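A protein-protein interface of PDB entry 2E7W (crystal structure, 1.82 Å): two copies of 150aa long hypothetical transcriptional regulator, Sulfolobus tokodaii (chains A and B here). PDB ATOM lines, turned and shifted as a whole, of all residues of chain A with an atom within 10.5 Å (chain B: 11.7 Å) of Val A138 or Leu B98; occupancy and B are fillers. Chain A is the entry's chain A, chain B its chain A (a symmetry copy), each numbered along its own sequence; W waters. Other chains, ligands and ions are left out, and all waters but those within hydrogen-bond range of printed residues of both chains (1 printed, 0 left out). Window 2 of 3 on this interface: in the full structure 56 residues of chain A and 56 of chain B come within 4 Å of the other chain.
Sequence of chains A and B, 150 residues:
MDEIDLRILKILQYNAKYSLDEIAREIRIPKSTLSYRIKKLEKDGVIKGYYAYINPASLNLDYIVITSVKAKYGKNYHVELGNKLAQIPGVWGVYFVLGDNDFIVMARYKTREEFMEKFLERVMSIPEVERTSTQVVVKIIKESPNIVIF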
ATOM      1  N   LEU A  61       2.552  10.592   0.404  1.00  0.00           N
ATOM      2  CA  LEU A  61       1.142  10.556   0.792  1.00  0.00           C
ATOM      3  C   LEU A  61       0.926   9.216   1.485  1.00  0.00           C
ATOM      4  O   LEU A  61       0.422   8.259   0.892  1.00  0.00           O
ATOM      5  CB  LEU A  61       0.253  10.684  -0.446  1.00  0.00           C
ATOM      6  CG  LEU A  61       0.326  12.063  -1.111  1.00  0.00           C
ATOM      7  CD1 LEU A  61      -0.421  12.053  -2.442  1.00  0.00           C
ATOM      8  CD2 LEU A  61      -0.252  13.105  -0.174  1.00  0.00           C
ATOM      9  N   ASP A  62       1.311   9.180   2.755  1.00  0.00           N
ATOM     10  CA  ASP A  62       1.256   7.977   3.572  1.00  0.00           C
ATOM     11  C   ASP A  62       0.006   7.805   4.433  1.00  0.00           C
ATOM     12  O   ASP A  62      -0.285   6.697   4.886  1.00  0.00           O
ATOM     13  CB  ASP A  62       2.510   7.944   4.452  1.00  0.00           C
ATOM     14  CG  ASP A  62       2.764   6.586   5.065  1.00  0.00           C
ATOM     15  OD1 ASP A  62       2.389   6.379   6.238  1.00  0.00           O
ATOM     16  OD2 ASP A  62       3.333   5.721   4.367  1.00  0.00           O
ATOM     17  N   TYR A  63      -0.729   8.888   4.659  1.00  0.00           N
ATOM     18  CA  TYR A  63      -1.939   8.823   5.479  1.00  0.00           C
ATOM     19  C   TYR A  63      -3.155   8.880   4.569  1.00  0.00           C
ATOM     20  O   TYR A  63      -3.621   9.964   4.208  1.00  0.00           O
ATOM     21  CB  TYR A  63      -1.977   9.991   6.461  1.00  0.00           C
ATOM     22  CG  TYR A  63      -2.473   9.592   7.831  1.00  0.00           C
ATOM     23  CD1 TYR A  63      -1.650   8.881   8.704  1.00  0.00           C
ATOM     24  CD2 TYR A  63      -3.769   9.900   8.242  1.00  0.00           C
ATOM     25  CE1 TYR A  63      -2.101   8.488   9.957  1.00  0.00           C
ATOM     26  CE2 TYR A  63      -4.235   9.508   9.498  1.00  0.00           C
ATOM     27  CZ  TYR A  63      -3.393   8.804  10.347  1.00  0.00           C
ATOM     28  OH  TYR A  63      -3.838   8.421  11.588  1.00  0.00           O
ATOM     29  N   ILE A  64      -3.661   7.704   4.214  1.00  0.00           N
ATOM     30  CA  ILE A  64      -4.796   7.566   3.303  1.00  0.00           C
ATOM     31  C   ILE A  64      -6.054   7.230   4.100  1.00  0.00           C
ATOM     32  O   ILE A  64      -6.051   6.304   4.914  1.00  0.00           O
ATOM     33  CB  ILE A  64      -4.491   6.452   2.273  1.00  0.00           C
ATOM     34  CG1 ILE A  64      -3.122   6.710   1.630  1.00  0.00           C
ATOM     35  CG2 ILE A  64      -5.582   6.380   1.219  1.00  0.00           C
ATOM     36  CD1 ILE A  64      -2.984   8.056   0.934  1.00  0.00           C
ATOM     37  N   VAL A  65      -7.125   7.980   3.857  1.00  0.00           N
ATOM     38  CA  VAL A  65      -8.363   7.797   4.600  1.00  0.00           C
ATOM     39  C   VAL A  65      -9.639   7.738   3.765  1.00  0.00           C
ATOM     40  O   VAL A  65      -9.713   8.298   2.675  1.00  0.00           O
ATOM     41  CB  VAL A  65      -8.527   8.936   5.636  1.00  0.00           C
ATOM     42  CG1 VAL A  65      -7.448   8.829   6.707  1.00  0.00           C
ATOM     43  CG2 VAL A  65      -8.420  10.296   4.936  1.00  0.00           C
ATOM     44  N   ILE A  66     -10.638   7.042   4.298  1.00  0.00           N
ATOM     45  CA  ILE A  66     -11.957   6.917   3.666  1.00  0.00           C
ATOM     46  C   ILE A  66     -12.899   7.243   4.817  1.00  0.00           C
ATOM     47  O   ILE A  66     -12.968   6.494   5.796  1.00  0.00           O
ATOM     48  CB  ILE A  66     -12.206   5.480   3.150  1.00  0.00           C
ATOM     49  CG1 ILE A  66     -11.177   5.135   2.061  1.00  0.00           C
ATOM     50  CG2 ILE A  66     -13.631   5.362   2.594  1.00  0.00           C
ATOM     51  CD1 ILE A  66     -11.318   3.722   1.497  1.00  0.00           C
ATOM     52  N   THR A  67     -13.600   8.371   4.719  1.00  0.00           N
ATOM     53  CA  THR A  67     -14.480   8.812   5.802  1.00  0.00           C
ATOM     54  C   THR A  67     -15.957   8.885   5.453  1.00  0.00           C
ATOM     55  O   THR A  67     -16.329   9.452   4.425  1.00  0.00           O
ATOM     56  CB  THR A  67     -14.061  10.224   6.310  1.00  0.00           C
ATOM     57  OG1 THR A  67     -12.703  10.191   6.763  1.00  0.00           O
ATOM     58  CG2 THR A  67     -14.950  10.682   7.458  1.00  0.00           C
ATOM     59  N   SER A  68     -16.794   8.318   6.322  1.00  0.00           N
ATOM     60  CA  SER A  68     -18.239   8.379   6.136  1.00  0.00           C
ATOM     61  C   SER A  68     -18.713   9.605   6.915  1.00  0.00           C
ATOM     62  O   SER A  68     -18.295   9.825   8.052  1.00  0.00           O
ATOM     63  CB  SER A  68     -18.911   7.118   6.687  1.00  0.00           C
ATOM     64  OG  SER A  68     -18.643   6.010   5.840  1.00  0.00           O
ATOM     65  N   ALA A 107      -9.613  10.701   0.730  1.00  0.00           N
ATOM     66  CA  ALA A 107      -8.586  11.738   0.803  1.00  0.00           C
ATOM     67  C   ALA A 107      -7.209  11.149   1.049  1.00  0.00           C
ATOM     68  O   ALA A 107      -7.078   9.992   1.467  1.00  0.00           O
ATOM     69  CB  ALA A 107      -8.926  12.735   1.907  1.00  0.00           C
ATOM     70  N   SER A 133     -16.995   8.833  10.482  1.00  0.00           N
ATOM     71  CA  SER A 133     -16.262   7.617  10.795  1.00  0.00           C
ATOM     72  C   SER A 133     -15.136   7.524   9.785  1.00  0.00           C
ATOM     73  O   SER A 133     -15.384   7.339   8.601  1.00  0.00           O
ATOM     74  CB  SER A 133     -17.158   6.386  10.674  1.00  0.00           C
ATOM     75  OG  SER A 133     -16.389   5.205  10.861  1.00  0.00           O
ATOM     76  N   THR A 134     -13.905   7.664  10.261  1.00  0.00           N
ATOM     77  CA  THR A 134     -12.735   7.603   9.393  1.00  0.00           C
ATOM     78  C   THR A 134     -12.070   6.235   9.437  1.00  0.00           C
ATOM     79  O   THR A 134     -11.686   5.753  10.506  1.00  0.00           O
ATOM     80  CB  THR A 134     -11.689   8.667   9.794  1.00  0.00           C
ATOM     81  OG1 THR A 134     -12.246   9.974   9.596  1.00  0.00           O
ATOM     82  CG2 THR A 134     -10.418   8.529   8.937  1.00  0.00           C
ATOM     83  N   GLN A 135     -11.953   5.619   8.265  1.00  0.00           N
ATOM     84  CA  GLN A 135     -11.314   4.315   8.105  1.00  0.00           C
ATOM     85  C   GLN A 135      -9.905   4.577   7.592  1.00  0.00           C
ATOM     86  O   GLN A 135      -9.734   5.142   6.516  1.00  0.00           O
ATOM     87  CB  GLN A 135     -12.060   3.481   7.064  1.00  0.00           C
ATOM     88  CG  GLN A 135     -13.525   3.315   7.363  1.00  0.00           C
ATOM     89  CD  GLN A 135     -13.745   2.564   8.643  1.00  0.00           C
ATOM     90  OE1 GLN A 135     -13.396   1.389   8.750  1.00  0.00           O
ATOM     91  NE2 GLN A 135     -14.315   3.236   9.633  1.00  0.00           N
ATOM     92  N   VAL A 136      -8.895   4.178   8.349  1.00  0.00           N
ATOM     93  CA  VAL A 136      -7.534   4.409   7.889  1.00  0.00           C
ATOM     94  C   VAL A 136      -7.089   3.287   6.952  1.00  0.00           C
ATOM     95  O   VAL A 136      -7.088   2.123   7.323  1.00  0.00           O
ATOM     96  CB  VAL A 136      -6.565   4.522   9.085  1.00  0.00           C
ATOM     97  CG1 VAL A 136      -5.140   4.695   8.589  1.00  0.00           C
ATOM     98  CG2 VAL A 136      -6.972   5.716   9.963  1.00  0.00           C
ATOM     99  N   VAL A 137      -6.739   3.648   5.720  1.00  0.00           N
ATOM    100  CA  VAL A 137      -6.281   2.666   4.745  1.00  0.00           C
ATOM    101  C   VAL A 137      -4.869   2.217   5.115  1.00  0.00           C
ATOM    102  O   VAL A 137      -3.950   3.033   5.176  1.00  0.00           O
ATOM    103  CB  VAL A 137      -6.261   3.269   3.321  1.00  0.00           C
ATOM    104  CG1 VAL A 137      -5.697   2.256   2.327  1.00  0.00           C
ATOM    105  CG2 VAL A 137      -7.675   3.680   2.918  1.00  0.00           C
ATOM    106  N   VAL A 138      -4.697   0.926   5.373  1.00  0.00           N
ATOM    107  CA  VAL A 138      -3.379   0.411   5.730  1.00  0.00           C
ATOM    108  C   VAL A 138      -2.776  -0.442   4.621  1.00  0.00           C
ATOM    109  O   VAL A 138      -1.633  -0.894   4.713  1.00  0.00           O
ATOM    110  CB  VAL A 138      -3.425  -0.384   7.050  1.00  0.00           C
ATOM    111  CG1 VAL A 138      -3.662   0.576   8.217  1.00  0.00           C
ATOM    112  CG2 VAL A 138      -4.512  -1.428   6.996  1.00  0.00           C
ATOM    113  N   LYS A 139      -3.552  -0.671   3.569  1.00  0.00           N
ATOM    114  CA  LYS A 139      -3.053  -1.420   2.429  1.00  0.00           C
ATOM    115  C   LYS A 139      -3.910  -1.163   1.204  1.00  0.00           C
ATOM    116  O   LYS A 139      -5.134  -1.273   1.256  1.00  0.00           O
ATOM    117  CB  LYS A 139      -3.003  -2.923   2.716  1.00  0.00           C
ATOM    118  CG  LYS A 139      -2.308  -3.703   1.608  1.00  0.00           C
ATOM    119  CD  LYS A 139      -1.730  -5.018   2.099  1.00  0.00           C
ATOM    120  CE  LYS A 139      -0.895  -5.678   1.012  1.00  0.00           C
ATOM    121  NZ  LYS A 139       0.240  -4.811   0.579  1.00  0.00           N
ATOM    122  N   ILE A 140      -3.257  -0.788   0.111  1.00  0.00           N
ATOM    123  CA  ILE A 140      -3.955  -0.551  -1.141  1.00  0.00           C
ATOM    124  C   ILE A 140      -3.660  -1.776  -1.999  1.00  0.00           C
ATOM    125  O   ILE A 140      -2.553  -1.922  -2.537  1.00  0.00           O
ATOM    126  CB  ILE A 140      -3.439   0.727  -1.845  1.00  0.00           C
ATOM    127  CG1 ILE A 140      -3.704   1.949  -0.962  1.00  0.00           C
ATOM    128  CG2 ILE A 140      -4.137   0.900  -3.190  1.00  0.00           C
ATOM    129  CD1 ILE A 140      -3.202   3.255  -1.545  1.00  0.00           C
ATOM    130  N   ILE A 141      -4.637  -2.672  -2.091  1.00  0.00           N
ATOM    131  CA  ILE A 141      -4.486  -3.895  -2.871  1.00  0.00           C
ATOM    132  C   ILE A 141      -4.578  -3.537  -4.349  1.00  0.00           C
ATOM    133  O   ILE A 141      -3.890  -4.124  -5.189  1.00  0.00           O
ATOM    134  CB  ILE A 141      -5.585  -4.940  -2.509  1.00  0.00           C
ATOM    135  CG1 ILE A 141      -5.379  -5.459  -1.080  1.00  0.00           C
ATOM    136  CG2 ILE A 141      -5.533  -6.116  -3.468  1.00  0.00           C
ATOM    137  CD1 ILE A 141      -5.708  -4.459   0.004  1.00  0.00           C
ATOM    138  N   LYS A 142      -5.420  -2.557  -4.657  1.00  0.00           N
ATOM    139  CA  LYS A 142      -5.596  -2.107  -6.031  1.00  0.00           C
ATOM    140  C   LYS A 142      -6.205  -0.715  -6.078  1.00  0.00           C
ATOM    141  O   LYS A 142      -7.098  -0.390  -5.302  1.00  0.00           O
ATOM    142  CB  LYS A 142      -6.508  -3.076  -6.790  1.00  0.00           C
ATOM    143  CG  LYS A 142      -6.704  -2.734  -8.266  1.00  0.00           C
ATOM    144  CD  LYS A 142      -7.650  -3.724  -8.931  1.00  0.00           C
ATOM    145  CE  LYS A 142      -7.758  -3.473 -10.431  1.00  0.00           C
ATOM    146  NZ  LYS A 142      -8.659  -4.472 -11.066  1.00  0.00           N
ATOM    147  N   SER B  68     -18.214  -3.067   1.408  1.00  0.00           N
ATOM    148  CA  SER B  68     -17.363  -3.457   2.526  1.00  0.00           C
ATOM    149  C   SER B  68     -17.428  -4.982   2.596  1.00  0.00           C
ATOM    150  O   SER B  68     -18.507  -5.567   2.497  1.00  0.00           O
ATOM    151  CB  SER B  68     -17.875  -2.851   3.836  1.00  0.00           C
ATOM    152  OG  SER B  68     -17.621  -1.454   3.863  1.00  0.00           O
ATOM    153  N   VAL B  69     -16.274  -5.618   2.756  1.00  0.00           N
ATOM    154  CA  VAL B  69     -16.206  -7.071   2.816  1.00  0.00           C
ATOM    155  C   VAL B  69     -15.375  -7.522   4.007  1.00  0.00           C
ATOM    156  O   VAL B  69     -14.195  -7.187   4.111  1.00  0.00           O
ATOM    157  CB  VAL B  69     -15.560  -7.648   1.538  1.00  0.00           C
ATOM    158  CG1 VAL B  69     -15.591  -9.172   1.584  1.00  0.00           C
ATOM    159  CG2 VAL B  69     -16.297  -7.131   0.298  1.00  0.00           C
ATOM    160  N   LYS B  70     -15.998  -8.282   4.900  1.00  0.00           N
ATOM    161  CA  LYS B  70     -15.313  -8.798   6.077  1.00  0.00           C
ATOM    162  C   LYS B  70     -14.839 -10.220   5.796  1.00  0.00           C
ATOM    163  O   LYS B  70     -15.566 -11.024   5.208  1.00  0.00           O
ATOM    164  CB  LYS B  70     -16.251  -8.773   7.287  1.00  0.00           C
ATOM    165  CG  LYS B  70     -16.583  -7.360   7.747  1.00  0.00           C
ATOM    166  CD  LYS B  70     -17.447  -7.344   8.998  1.00  0.00           C
ATOM    167  CE  LYS B  70     -17.534  -5.933   9.564  1.00  0.00           C
ATOM    168  NZ  LYS B  70     -17.930  -4.947   8.521  1.00  0.00           N
ATOM    169  N   TYR B  73     -11.205 -15.080   9.973  1.00  0.00           N
ATOM    170  CA  TYR B  73      -9.868 -15.019  10.555  1.00  0.00           C
ATOM    171  C   TYR B  73      -9.199 -16.385  10.506  1.00  0.00           C
ATOM    172  O   TYR B  73      -9.872 -17.413  10.478  1.00  0.00           O
ATOM    173  CB  TYR B  73      -9.939 -14.523  11.999  1.00  0.00           C
ATOM    174  CG  TYR B  73     -10.161 -13.031  12.098  1.00  0.00           C
ATOM    175  CD1 TYR B  73     -11.400 -12.464  11.797  1.00  0.00           C
ATOM    176  CD2 TYR B  73      -9.108 -12.181  12.418  1.00  0.00           C
ATOM    177  CE1 TYR B  73     -11.577 -11.077  11.805  1.00  0.00           C
ATOM    178  CE2 TYR B  73      -9.273 -10.797  12.429  1.00  0.00           C
ATOM    179  CZ  TYR B  73     -10.507 -10.255  12.119  1.00  0.00           C
ATOM    180  OH  TYR B  73     -10.649  -8.888  12.109  1.00  0.00           O
ATOM    181  N   HIS B  78      -7.481 -13.586   4.953  1.00  0.00           N
ATOM    182  CA  HIS B  78      -7.494 -12.157   4.654  1.00  0.00           C
ATOM    183  C   HIS B  78      -6.730 -11.779   3.388  1.00  0.00           C
ATOM    184  O   HIS B  78      -7.307 -11.227   2.453  1.00  0.00           O
ATOM    185  CB  HIS B  78      -6.960 -11.349   5.844  1.00  0.00           C
ATOM    186  CG  HIS B  78      -7.997 -11.061   6.889  1.00  0.00           C
ATOM    187  ND1 HIS B  78      -8.481 -12.026   7.746  1.00  0.00           N
ATOM    188  CD2 HIS B  78      -8.669  -9.922   7.184  1.00  0.00           C
ATOM    189  CE1 HIS B  78      -9.411 -11.495   8.522  1.00  0.00           C
ATOM    190  NE2 HIS B  78      -9.545 -10.219   8.200  1.00  0.00           N
ATOM    191  N   VAL B  79      -5.436 -12.082   3.350  1.00  0.00           N
ATOM    192  CA  VAL B  79      -4.616 -11.756   2.186  1.00  0.00           C
ATOM    193  C   VAL B  79      -5.158 -12.355   0.894  1.00  0.00           C
ATOM    194  O   VAL B  79      -5.215 -11.684  -0.139  1.00  0.00           O
ATOM    195  CB  VAL B  79      -3.163 -12.240   2.372  1.00  0.00           C
ATOM    196  CG1 VAL B  79      -2.396 -12.098   1.065  1.00  0.00           C
ATOM    197  CG2 VAL B  79      -2.486 -11.426   3.463  1.00  0.00           C
ATOM    198  N   VAL B  94      -9.418  -1.643  -4.275  1.00  0.00           N
ATOM    199  CA  VAL B  94      -9.547  -2.579  -3.158  1.00  0.00           C
ATOM    200  C   VAL B  94      -8.595  -2.091  -2.077  1.00  0.00           C
ATOM    201  O   VAL B  94      -7.385  -1.980  -2.303  1.00  0.00           O
ATOM    202  CB  VAL B  94      -9.178  -4.036  -3.539  1.00  0.00           C
ATOM    203  CG1 VAL B  94      -9.285  -4.924  -2.309  1.00  0.00           C
ATOM    204  CG2 VAL B  94     -10.112  -4.551  -4.632  1.00  0.00           C
ATOM    205  N   TYR B  95      -9.152  -1.780  -0.909  1.00  0.00           N
ATOM    206  CA  TYR B  95      -8.362  -1.268   0.203  1.00  0.00           C
ATOM    207  C   TYR B  95      -8.652  -2.050   1.470  1.00  0.00           C
ATOM    208  O   TYR B  95      -9.771  -2.515   1.661  1.00  0.00           O
ATOM    209  CB  TYR B  95      -8.741   0.189   0.508  1.00  0.00           C
ATOM    210  CG  TYR B  95      -8.775   1.130  -0.672  1.00  0.00           C
ATOM    211  CD1 TYR B  95      -9.952   1.336  -1.397  1.00  0.00           C
ATOM    212  CD2 TYR B  95      -7.636   1.837  -1.048  1.00  0.00           C
ATOM    213  CE1 TYR B  95      -9.988   2.231  -2.468  1.00  0.00           C
ATOM    214  CE2 TYR B  95      -7.661   2.732  -2.115  1.00  0.00           C
ATOM    215  CZ  TYR B  95      -8.838   2.925  -2.821  1.00  0.00           C
ATOM    216  OH  TYR B  95      -8.866   3.818  -3.875  1.00  0.00           O
ATOM    217  N   PHE B  96      -7.651  -2.217   2.330  1.00  0.00           N
ATOM    218  CA  PHE B  96      -7.936  -2.842   3.610  1.00  0.00           C
ATOM    219  C   PHE B  96      -7.821  -1.666   4.569  1.00  0.00           C
ATOM    220  O   PHE B  96      -6.833  -0.928   4.546  1.00  0.00           O
ATOM    221  CB  PHE B  96      -6.952  -3.941   3.990  1.00  0.00           C
ATOM    222  CG  PHE B  96      -7.345  -4.651   5.251  1.00  0.00           C
ATOM    223  CD1 PHE B  96      -6.895  -4.203   6.486  1.00  0.00           C
ATOM    224  CD2 PHE B  96      -8.252  -5.708   5.210  1.00  0.00           C
ATOM    225  CE1 PHE B  96      -7.342  -4.792   7.668  1.00  0.00           C
ATOM    226  CE2 PHE B  96      -8.710  -6.306   6.386  1.00  0.00           C
ATOM    227  CZ  PHE B  96      -8.254  -5.845   7.617  1.00  0.00           C
ATOM    228  N   VAL B  97      -8.836  -1.481   5.404  1.00  0.00           N
ATOM    229  CA  VAL B  97      -8.855  -0.337   6.302  1.00  0.00           C
ATOM    230  C   VAL B  97      -9.038  -0.701   7.767  1.00  0.00           C
ATOM    231  O   VAL B  97      -9.572  -1.760   8.093  1.00  0.00           O
ATOM    232  CB  VAL B  97      -9.996   0.636   5.905  1.00  0.00           C
ATOM    233  CG1 VAL B  97      -9.860   1.022   4.439  1.00  0.00           C
ATOM    234  CG2 VAL B  97     -11.363  -0.022   6.124  1.00  0.00           C
ATOM    235  N   LEU B  98      -8.582   0.187   8.643  1.00  0.00           N
ATOM    236  CA  LEU B  98      -8.752  -0.030  10.073  1.00  0.00           C
ATOM    237  C   LEU B  98     -10.109   0.564  10.431  1.00  0.00           C
ATOM    238  O   LEU B  98     -10.780   1.136   9.570  1.00  0.00           O
ATOM    239  CB  LEU B  98      -7.623   0.636  10.848  1.00  0.00           C
ATOM    240  CG  LEU B  98      -6.253   0.050  10.493  1.00  0.00           C
ATOM    241  CD1 LEU B  98      -5.184   0.713  11.349  1.00  0.00           C
ATOM    242  CD2 LEU B  98      -6.260  -1.464  10.717  1.00  0.00           C
ATOM    243  N   GLY B  99     -10.526   0.431  11.681  1.00  0.00           N
ATOM    244  CA  GLY B  99     -11.839   0.930  12.054  1.00  0.00           C
ATOM    245  C   GLY B  99     -12.760  -0.268  11.893  1.00  0.00           C
ATOM    246  O   GLY B  99     -13.041  -0.965  12.865  1.00  0.00           O
ATOM    247  N   ASP B 100     -13.218  -0.521  10.669  1.00  0.00           N
ATOM    248  CA  ASP B 100     -14.069  -1.683  10.416  1.00  0.00           C
ATOM    249  C   ASP B 100     -13.181  -2.909  10.226  1.00  0.00           C
ATOM    250  O   ASP B 100     -13.671  -4.037  10.215  1.00  0.00           O
ATOM    251  CB  ASP B 100     -14.912  -1.502   9.148  1.00  0.00           C
ATOM    252  CG  ASP B 100     -15.983  -0.436   9.292  1.00  0.00           C
ATOM    253  OD1 ASP B 100     -16.458  -0.212  10.426  1.00  0.00           O
ATOM    254  OD2 ASP B 100     -16.361   0.162   8.256  1.00  0.00           O
ATOM    255  N   ASN B 101     -11.877  -2.680  10.070  1.00  0.00           N
ATOM    256  CA  ASN B 101     -10.914  -3.761   9.856  1.00  0.00           C
ATOM    257  C   ASN B 101     -11.415  -4.736   8.793  1.00  0.00           C
ATOM    258  O   ASN B 101     -11.593  -5.937   9.045  1.00  0.00           O
ATOM    259  CB  ASN B 101     -10.626  -4.517  11.165  1.00  0.00           C
ATOM    260  CG  ASN B 101      -9.718  -3.737  12.111  1.00  0.00           C
ATOM    261  OD1 ASN B 101      -9.037  -4.326  12.961  1.00  0.00           O
ATOM    262  ND2 ASN B 101      -9.715  -2.413  11.985  1.00  0.00           N
ATOM    263  N   ASP B 102     -11.648  -4.210   7.599  1.00  0.00           N
ATOM    264  CA  ASP B 102     -12.133  -5.025   6.497  1.00  0.00           C
ATOM    265  C   ASP B 102     -11.711  -4.418   5.171  1.00  0.00           C
ATOM    266  O   ASP B 102     -10.900  -3.499   5.141  1.00  0.00           O
ATOM    267  CB  ASP B 102     -13.662  -5.166   6.568  1.00  0.00           C
ATOM    268  CG  ASP B 102     -14.393  -3.830   6.479  1.00  0.00           C
ATOM    269  OD1 ASP B 102     -13.782  -2.811   6.099  1.00  0.00           O
ATOM    270  OD2 ASP B 102     -15.604  -3.805   6.784  1.00  0.00           O
ATOM    271  N   PHE B 103     -12.245  -4.950   4.075  1.00  0.00           N
ATOM    272  CA  PHE B 103     -11.912  -4.445   2.749  1.00  0.00           C
ATOM    273  C   PHE B 103     -13.006  -3.518   2.247  1.00  0.00           C
ATOM    274  O   PHE B 103     -14.184  -3.731   2.531  1.00  0.00           O
ATOM    275  CB  PHE B 103     -11.795  -5.598   1.746  1.00  0.00           C
ATOM    276  CG  PHE B 103     -10.640  -6.515   1.993  1.00  0.00           C
ATOM    277  CD1 PHE B 103      -9.362  -6.175   1.563  1.00  0.00           C
ATOM    278  CD2 PHE B 103     -10.831  -7.729   2.648  1.00  0.00           C
ATOM    279  CE1 PHE B 103      -8.288  -7.033   1.780  1.00  0.00           C
ATOM    280  CE2 PHE B 103      -9.761  -8.595   2.871  1.00  0.00           C
ATOM    281  CZ  PHE B 103      -8.487  -8.241   2.432  1.00  0.00           C
ATOM    282  N   ILE B 104     -12.602  -2.486   1.513  1.00  0.00           N
ATOM    283  CA  ILE B 104     -13.537  -1.564   0.885  1.00  0.00           C
ATOM    284  C   ILE B 104     -13.232  -1.749  -0.599  1.00  0.00           C
ATOM    285  O   ILE B 104     -12.091  -1.600  -1.030  1.00  0.00           O
ATOM    286  CB  ILE B 104     -13.308  -0.101   1.322  1.00  0.00           C
ATOM    287  CG1 ILE B 104     -13.712   0.050   2.797  1.00  0.00           C
ATOM    288  CG2 ILE B 104     -14.145   0.842   0.454  1.00  0.00           C
ATOM    289  CD1 ILE B 104     -13.717   1.469   3.312  1.00  0.00           C
HETATM  290  O   HOH W   1     -15.257   2.043  11.964  1.00  0.00           O
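The backbone carbonyl oxygen (O) of Leu B98 sits close to the side-chain amide oxygen (OE1) of Gln A135. The backbone NH (N) of Asp B100 is in hydrogen-bond range of the side-chain amide oxygen (OE1) of Gln A135. N of Leu B98 lies within hydrogen-bond range of O of Val A136, at 2.8 Å. The backbone NH (N) of Val A138 is in hydrogen-bond range of the backbone carbonyl oxygen (O) of Phe B96 (2.9 Å). O of Lys A139 lies within hydrogen-bond range of N of Phe B96 (2.9 Å). The backbone carbonyl oxygen (O) of Val B94 is in hydrogen-bond range of the backbone NH (N) of Ile A141 (2.8 Å). The backbone carbonyl oxygen (O) of Lys A142 sits at hydrogen-bond distance from the backbone NH (N) of Val B94, 2.8 Å away.
N of Val A137 is in hydrogen-bond range of O of Ile A64 (2.9 Å). N of Gln A135 is in hydrogen-bond range of O of Ile A66. The side-chain amide nitrogen (NE2) of Gln A135 sits at hydrogen-bond distance from the side-chain hydroxyl (OG) of Ser A133. O of Tyr B95 lies within hydrogen-bond range of N of Ile B104. N of Val B97 lies within hydrogen-bond range of O of Asp B102, 2.9 Å away. The side-chain amide nitrogen (ND2) of Asn B101 lies close to the backbone NH (N) of Gly B99, 3.0 Å away.
CD1 of Tyr B95 touches CD1 of Ile A66, 3.99 Å away. CD1 of Ile A66 touches CD1 of Ile B104, 3.8 Å away. Gln A135 touches Val B97. O of Val A136 touches CA of Val B97, at 3.2 Å. Val A137 touches Phe B96. CG1 of Val B97 touches CG2 of Val A137, 3.8 Å away. Val A138 touches Leu B98 (CG1 to CD1, 3.5 Å). Ile A140 touches Val B94 (C to O, 3.7 Å). CG1 of Ile A140 touches CD2 of Tyr B95, at 3.9 Å. CD1 of Ile A141 touches N of Phe B96 (3.8 Å).
Of the printed residues of chain B, Ile A66 touches Tyr B95 and Ile B104. Of chain B, only Val B97, Leu B98, Gly B99 and Asp B100 come within 4 Å of Gln A135. Val A136 touches just these residues of chain B: Val B97 (3.2 Å) and Leu B98 (2.8 Å). Of chain B, only Tyr B95 (3.9 Å), Phe B96 (3.6 Å) and Val B97 (3.8 Å) come within 4 Å of Val A137. Val A138 touches two residues of chain B. Of chain B, only Tyr B95 and Phe B96 come within 4 Å of Lys A139. Of the printed residues of chain B, Ile A140 touches Val B94 and Tyr B95. Lys B70 touches none of the printed residues of chain A. Val B97 touches three residues of chain A. Leu B98 touches just these residues of chain A: Gln A135 (2.8 Å), Val A136 (2.8 Å) and Val A138 (3.5 Å). Of chain A, only Gln A135 comes within 4 Å of Gly B99. Of chain A, only Gln A135 (2.7 Å) comes within 4 Å of Asp B100. Asn B101 touches none of the printed residues of chain A. Of the printed residues of chain A, Ile B104 touches Ile A66 (3.8 Å). The nearest residue of chain A that does not touch Leu B98 is Thr A134 (4.8 Å). The nearest printed residue of chain B that does not touch Ile A140 is Phe B96 (5.1 Å).
Of the 19 printed residues of chain A, 9 touch a printed residue of chain B. Along chain A the printed residues that touch a printed residue of chain B span positions 66 to 142. Printed residues of chain B that touch a printed residue of chain A: Val B94, Tyr B95, Phe B96, Val B97, Leu B98, Gly B99, Asp B100 and Ile B104. Hydrophobic or aromatic side chains of chain B within 4 Å of the printed part of chain A: Val B94, Tyr B95, Phe B96, Val B97, Leu B98 and Ile B104. Among the printed residues, 20 pairs touch across the chains.
1 position is printed for both chains. Of the 20 pairs that touch across the chains among the printed residues, none has its exchanged pair printed and touching as well.
Water W1 bridges the side-chain amide nitrogen (NE2) of Gln A135 (2.8 Å) and the side-chain carboxylate (OD1) of Asp B100 (3.0 Å).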
